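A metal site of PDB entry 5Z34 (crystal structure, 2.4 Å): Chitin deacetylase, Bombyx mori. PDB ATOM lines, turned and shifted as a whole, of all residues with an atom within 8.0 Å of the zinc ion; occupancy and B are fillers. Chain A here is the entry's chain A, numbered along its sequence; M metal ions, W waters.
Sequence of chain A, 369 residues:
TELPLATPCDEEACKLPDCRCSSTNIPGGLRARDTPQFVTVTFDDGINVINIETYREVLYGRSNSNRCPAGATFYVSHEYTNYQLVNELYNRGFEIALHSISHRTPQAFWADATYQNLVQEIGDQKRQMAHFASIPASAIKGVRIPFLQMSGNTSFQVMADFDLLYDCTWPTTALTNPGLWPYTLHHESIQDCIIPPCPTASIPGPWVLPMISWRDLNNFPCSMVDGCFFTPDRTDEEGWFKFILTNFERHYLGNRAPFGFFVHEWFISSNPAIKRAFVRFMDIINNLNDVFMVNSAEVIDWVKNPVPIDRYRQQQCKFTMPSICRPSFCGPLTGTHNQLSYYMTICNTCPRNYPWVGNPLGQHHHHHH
The backbone carbonyl oxygen (O) of Arg 144 lies within hydrogen-bond range of a ring nitrogen (ND1) of His 99 (2.9 Å). The backbone NH (N) of His 99 lies within hydrogen-bond range of the backbone carbonyl oxygen (O) of Val 76 (3.0 Å). The backbone NH (N) of His 103 lies within hydrogen-bond range of the side-chain hydroxyl (OG) of Ser 100, 3.0 Å away. The backbone NH (N) of Asp 45 sits at hydrogen-bond distance from the backbone carbonyl oxygen (O) of Tyr 75.
A ring nitrogen (NE2) of His 99 binds the zinc ion (2.0 Å). NE2 of His 103 binds the zinc ion. OD1 of Asp 45 is bound to the zinc ion (2.2 Å). The zinc ion is bound by water W1 (2.5 Å). The zinc ion has four donor atoms within binding distance.
Of the 17 residues printed, 3 come within 4 Å of the zinc ion.
Water W1 lies within hydrogen-bond range of OD2 of Asp 44 and NE2 of His 264.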
ATOM      1  N   PHE A  43      23.211  25.948 -14.437  1.00  0.00           N
ATOM      2  CA  PHE A  43      23.129  25.248 -15.709  1.00  0.00           C
ATOM      3  C   PHE A  43      23.622  26.165 -16.818  1.00  0.00           C
ATOM      4  O   PHE A  43      23.210  27.327 -16.898  1.00  0.00           O
ATOM      5  CB  PHE A  43      21.688  24.785 -15.988  1.00  0.00           C
ATOM      6  CG  PHE A  43      21.154  23.790 -14.988  1.00  0.00           C
ATOM      7  CD1 PHE A  43      21.442  22.439 -15.120  1.00  0.00           C
ATOM      8  CD2 PHE A  43      20.359  24.203 -13.932  1.00  0.00           C
ATOM      9  CE1 PHE A  43      20.945  21.516 -14.208  1.00  0.00           C
ATOM     10  CE2 PHE A  43      19.869  23.280 -13.014  1.00  0.00           C
ATOM     11  CZ  PHE A  43      20.166  21.935 -13.155  1.00  0.00           C
ATOM     12  N   ASP A  44      24.459  25.651 -17.690  1.00  0.00           N
ATOM     13  CA  ASP A  44      25.036  26.410 -18.739  1.00  0.00           C
ATOM     14  C   ASP A  44      24.268  26.272 -20.038  1.00  0.00           C
ATOM     15  O   ASP A  44      23.554  25.364 -20.231  1.00  0.00           O
ATOM     16  CB  ASP A  44      26.512  26.098 -18.851  1.00  0.00           C
ATOM     17  CG  ASP A  44      27.353  26.746 -17.825  1.00  0.00           C
ATOM     18  OD1 ASP A  44      26.849  27.312 -16.914  1.00  0.00           O
ATOM     19  OD2 ASP A  44      28.555  26.660 -17.892  1.00  0.00           O
ATOM     20  N   ASP A  45      24.485  27.201 -20.934  1.00  0.00           N
ATOM     21  CA  ASP A  45      24.042  27.169 -22.304  1.00  0.00           C
ATOM     22  C   ASP A  45      22.544  27.216 -22.519  1.00  0.00           C
ATOM     23  O   ASP A  45      21.827  27.370 -21.633  1.00  0.00           O
ATOM     24  CB  ASP A  45      24.559  25.928 -23.045  1.00  0.00           C
ATOM     25  CG  ASP A  45      26.051  25.693 -22.893  1.00  0.00           C
ATOM     26  OD1 ASP A  45      26.805  26.637 -22.557  1.00  0.00           O
ATOM     27  OD2 ASP A  45      26.479  24.538 -23.132  1.00  0.00           O
ATOM     28  N   GLY A  46      22.127  27.106 -23.778  1.00  0.00           N
ATOM     29  CA  GLY A  46      20.755  27.333 -24.228  1.00  0.00           C
ATOM     30  C   GLY A  46      19.517  26.682 -23.631  1.00  0.00           C
ATOM     31  O   GLY A  46      19.524  25.499 -23.287  1.00  0.00           O
ATOM     32  N   TYR A  75      23.134  30.268 -16.715  1.00  0.00           N
ATOM     33  CA  TYR A  75      24.044  31.020 -17.574  1.00  0.00           C
ATOM     34  C   TYR A  75      23.639  30.725 -19.016  1.00  0.00           C
ATOM     35  O   TYR A  75      24.035  29.705 -19.597  1.00  0.00           O
ATOM     36  CB  TYR A  75      25.485  30.646 -17.283  1.00  0.00           C
ATOM     37  CG  TYR A  75      25.913  31.091 -15.894  1.00  0.00           C
ATOM     38  CD1 TYR A  75      26.236  32.416 -15.628  1.00  0.00           C
ATOM     39  CD2 TYR A  75      25.960  30.169 -14.840  1.00  0.00           C
ATOM     40  CE1 TYR A  75      26.608  32.823 -14.366  1.00  0.00           C
ATOM     41  CE2 TYR A  75      26.337  30.566 -13.568  1.00  0.00           C
ATOM     42  CZ  TYR A  75      26.656  31.902 -13.341  1.00  0.00           C
ATOM     43  OH  TYR A  75      27.020  32.302 -12.070  1.00  0.00           O
ATOM     44  N   VAL A  76      22.849  31.620 -19.587  1.00  0.00           N
ATOM     45  CA  VAL A  76      22.154  31.372 -20.848  1.00  0.00           C
ATOM     46  C   VAL A  76      22.953  31.963 -21.995  1.00  0.00           C
ATOM     47  O   VAL A  76      23.307  33.158 -21.964  1.00  0.00           O
ATOM     48  CB  VAL A  76      20.731  31.961 -20.806  1.00  0.00           C
ATOM     49  CG1 VAL A  76      19.987  31.640 -22.095  1.00  0.00           C
ATOM     50  CG2 VAL A  76      19.976  31.424 -19.594  1.00  0.00           C
ATOM     51  N   SER A  77      23.219  31.155 -23.012  1.00  0.00           N
ATOM     52  CA  SER A  77      23.753  31.623 -24.276  1.00  0.00           C
ATOM     53  C   SER A  77      22.614  31.761 -25.290  1.00  0.00           C
ATOM     54  O   SER A  77      21.597  31.071 -25.205  1.00  0.00           O
ATOM     55  CB  SER A  77      24.849  30.694 -24.812  1.00  0.00           C
ATOM     56  OG  SER A  77      24.416  29.347 -24.832  1.00  0.00           O
ATOM     57  N   HIS A  99      25.894  34.049 -20.693  1.00  0.00           N
ATOM     58  CA  HIS A  99      26.860  33.085 -21.177  1.00  0.00           C
ATOM     59  C   HIS A  99      27.127  33.372 -22.651  1.00  0.00           C
ATOM     60  O   HIS A  99      27.446  32.496 -23.369  1.00  0.00           O
ATOM     61  CB  HIS A  99      26.329  31.656 -21.044  1.00  0.00           C
ATOM     62  CG  HIS A  99      27.339  30.548 -21.169  1.00  0.00           C
ATOM     63  ND1 HIS A  99      28.576  30.574 -20.606  1.00  0.00           N
ATOM     64  CD2 HIS A  99      27.229  29.327 -21.725  1.00  0.00           C
ATOM     65  CE1 HIS A  99      29.207  29.460 -20.857  1.00  0.00           C
ATOM     66  NE2 HIS A  99      28.413  28.679 -21.558  1.00  0.00           N
ATOM     67  N   SER A 100      26.975  34.615 -23.067  1.00  0.00           N
ATOM     68  CA  SER A 100      27.320  35.177 -24.390  1.00  0.00           C
ATOM     69  C   SER A 100      26.315  34.988 -25.481  1.00  0.00           C
ATOM     70  O   SER A 100      25.535  34.142 -25.410  1.00  0.00           O
ATOM     71  CB  SER A 100      28.692  34.770 -24.847  1.00  0.00           C
ATOM     72  OG  SER A 100      28.674  33.565 -25.499  1.00  0.00           O
ATOM     73  N   HIS A 103      28.754  32.074 -28.114  1.00  0.00           N
ATOM     74  CA  HIS A 103      29.419  30.899 -27.529  1.00  0.00           C
ATOM     75  C   HIS A 103      30.405  30.289 -28.518  1.00  0.00           C
ATOM     76  O   HIS A 103      30.617  29.081 -28.542  1.00  0.00           O
ATOM     77  CB  HIS A 103      28.403  29.846 -27.064  1.00  0.00           C
ATOM     78  CG  HIS A 103      28.915  28.946 -25.987  1.00  0.00           C
ATOM     79  ND1 HIS A 103      30.064  28.193 -26.119  1.00  0.00           N
ATOM     80  CD2 HIS A 103      28.426  28.675 -24.745  1.00  0.00           C
ATOM     81  CE1 HIS A 103      30.262  27.501 -25.012  1.00  0.00           C
ATOM     82  NE2 HIS A 103      29.286  27.771 -24.159  1.00  0.00           N
ATOM     83  N   ARG A 144      29.151  34.165 -16.992  1.00  0.00           N
ATOM     84  CA  ARG A 144      30.103  33.057 -17.085  1.00  0.00           C
ATOM     85  C   ARG A 144      30.616  33.014 -18.507  1.00  0.00           C
ATOM     86  O   ARG A 144      29.833  32.868 -19.456  1.00  0.00           O
ATOM     87  CB  ARG A 144      29.446  31.718 -16.702  1.00  0.00           C
ATOM     88  CG  ARG A 144      30.338  30.500 -16.953  1.00  0.00           C
ATOM     89  CD  ARG A 144      29.815  29.265 -16.243  1.00  0.00           C
ATOM     90  NE  ARG A 144      29.994  29.352 -14.792  1.00  0.00           N
ATOM     91  CZ  ARG A 144      29.349  28.596 -13.918  1.00  0.00           C
ATOM     92  NH1 ARG A 144      28.484  27.695 -14.359  1.00  0.00           N
ATOM     93  NH2 ARG A 144      29.556  28.738 -12.616  1.00  0.00           N
ATOM     94  N   ILE A 145      31.929  33.161 -18.684  1.00  0.00           N
ATOM     95  CA  ILE A 145      32.494  33.171 -20.034  1.00  0.00           C
ATOM     96  C   ILE A 145      32.504  31.745 -20.592  1.00  0.00           C
ATOM     97  O   ILE A 145      32.790  30.796 -19.825  1.00  0.00           O
ATOM     98  CB  ILE A 145      33.895  33.770 -20.031  1.00  0.00           C
ATOM     99  CG1 ILE A 145      33.899  35.130 -19.335  1.00  0.00           C
ATOM    100  CG2 ILE A 145      34.398  33.939 -21.463  1.00  0.00           C
ATOM    101  CD1 ILE A 145      35.281  35.725 -19.183  1.00  0.00           C
ATOM    102  N   PRO A 146      32.191  31.537 -21.863  1.00  0.00           N
ATOM    103  CA  PRO A 146      32.245  30.190 -22.446  1.00  0.00           C
ATOM    104  C   PRO A 146      33.567  29.486 -22.200  1.00  0.00           C
ATOM    105  O   PRO A 146      34.620  30.115 -22.113  1.00  0.00           O
ATOM    106  CB  PRO A 146      32.024  30.447 -23.947  1.00  0.00           C
ATOM    107  CG  PRO A 146      31.160  31.662 -23.969  1.00  0.00           C
ATOM    108  CD  PRO A 146      31.559  32.509 -22.780  1.00  0.00           C
ATOM    109  N   PHE A 147      33.486  28.155 -22.082  1.00  0.00           N
ATOM    110  CA  PHE A 147      34.647  27.272 -21.896  1.00  0.00           C
ATOM    111  C   PHE A 147      35.412  27.587 -20.613  1.00  0.00           C
ATOM    112  O   PHE A 147      36.554  27.133 -20.465  1.00  0.00           O
ATOM    113  CB  PHE A 147      35.608  27.340 -23.085  1.00  0.00           C
ATOM    114  CG  PHE A 147      34.947  27.154 -24.402  1.00  0.00           C
ATOM    115  CD1 PHE A 147      34.510  25.895 -24.803  1.00  0.00           C
ATOM    116  CD2 PHE A 147      34.745  28.231 -25.255  1.00  0.00           C
ATOM    117  CE1 PHE A 147      33.878  25.722 -26.022  1.00  0.00           C
ATOM    118  CE2 PHE A 147      34.115  28.068 -26.477  1.00  0.00           C
ATOM    119  CZ  PHE A 147      33.692  26.811 -26.863  1.00  0.00           C
ATOM    120  N   LEU A 148      34.807  28.344 -19.703  1.00  0.00           N
ATOM    121  CA  LEU A 148      35.493  28.763 -18.478  1.00  0.00           C
ATOM    122  C   LEU A 148      36.789  29.492 -18.812  1.00  0.00           C
ATOM    123  O   LEU A 148      37.764  29.442 -18.070  1.00  0.00           O
ATOM    124  CB  LEU A 148      35.743  27.567 -17.562  1.00  0.00           C
ATOM    125  CG  LEU A 148      34.592  26.978 -16.743  1.00  0.00           C
ATOM    126  CD1 LEU A 148      33.447  26.527 -17.633  1.00  0.00           C
ATOM    127  CD2 LEU A 148      35.074  25.818 -15.913  1.00  0.00           C
ATOM    128  N   MET A 224      33.387  21.643 -12.717  1.00  0.00           N
ATOM    129  CA  MET A 224      32.006  21.306 -12.999  1.00  0.00           C
ATOM    130  C   MET A 224      31.790  19.808 -12.782  1.00  0.00           C
ATOM    131  O   MET A 224      32.700  18.997 -12.978  1.00  0.00           O
ATOM    132  CB  MET A 224      31.645  21.747 -14.402  1.00  0.00           C
ATOM    133  CG  MET A 224      31.874  23.245 -14.575  1.00  0.00           C
ATOM    134  SD  MET A 224      31.258  23.919 -16.112  1.00  0.00           S
ATOM    135  CE  MET A 224      29.506  23.530 -16.034  1.00  0.00           C
ATOM    136  N   HIS A 264      26.020  20.969 -16.941  1.00  0.00           N
ATOM    137  CA  HIS A 264      25.151  21.070 -18.115  1.00  0.00           C
ATOM    138  C   HIS A 264      23.992  20.094 -17.941  1.00  0.00           C
ATOM    139  O   HIS A 264      24.176  19.000 -17.400  1.00  0.00           O
ATOM    140  CB  HIS A 264      25.910  20.743 -19.401  1.00  0.00           C
ATOM    141  CG  HIS A 264      27.104  21.622 -19.659  1.00  0.00           C
ATOM    142  ND1 HIS A 264      28.317  21.412 -19.047  1.00  0.00           N
ATOM    143  CD2 HIS A 264      27.264  22.681 -20.481  1.00  0.00           C
ATOM    144  CE1 HIS A 264      29.183  22.325 -19.473  1.00  0.00           C
ATOM    145  NE2 HIS A 264      28.565  23.107 -20.341  1.00  0.00           N
HETATM  146 ZN    ZN M   1      28.926  26.893 -22.240  1.00  0.00          ZN
HETATM  147  O   HOH W   1      30.090  26.177 -20.140  1.00  0.00           O
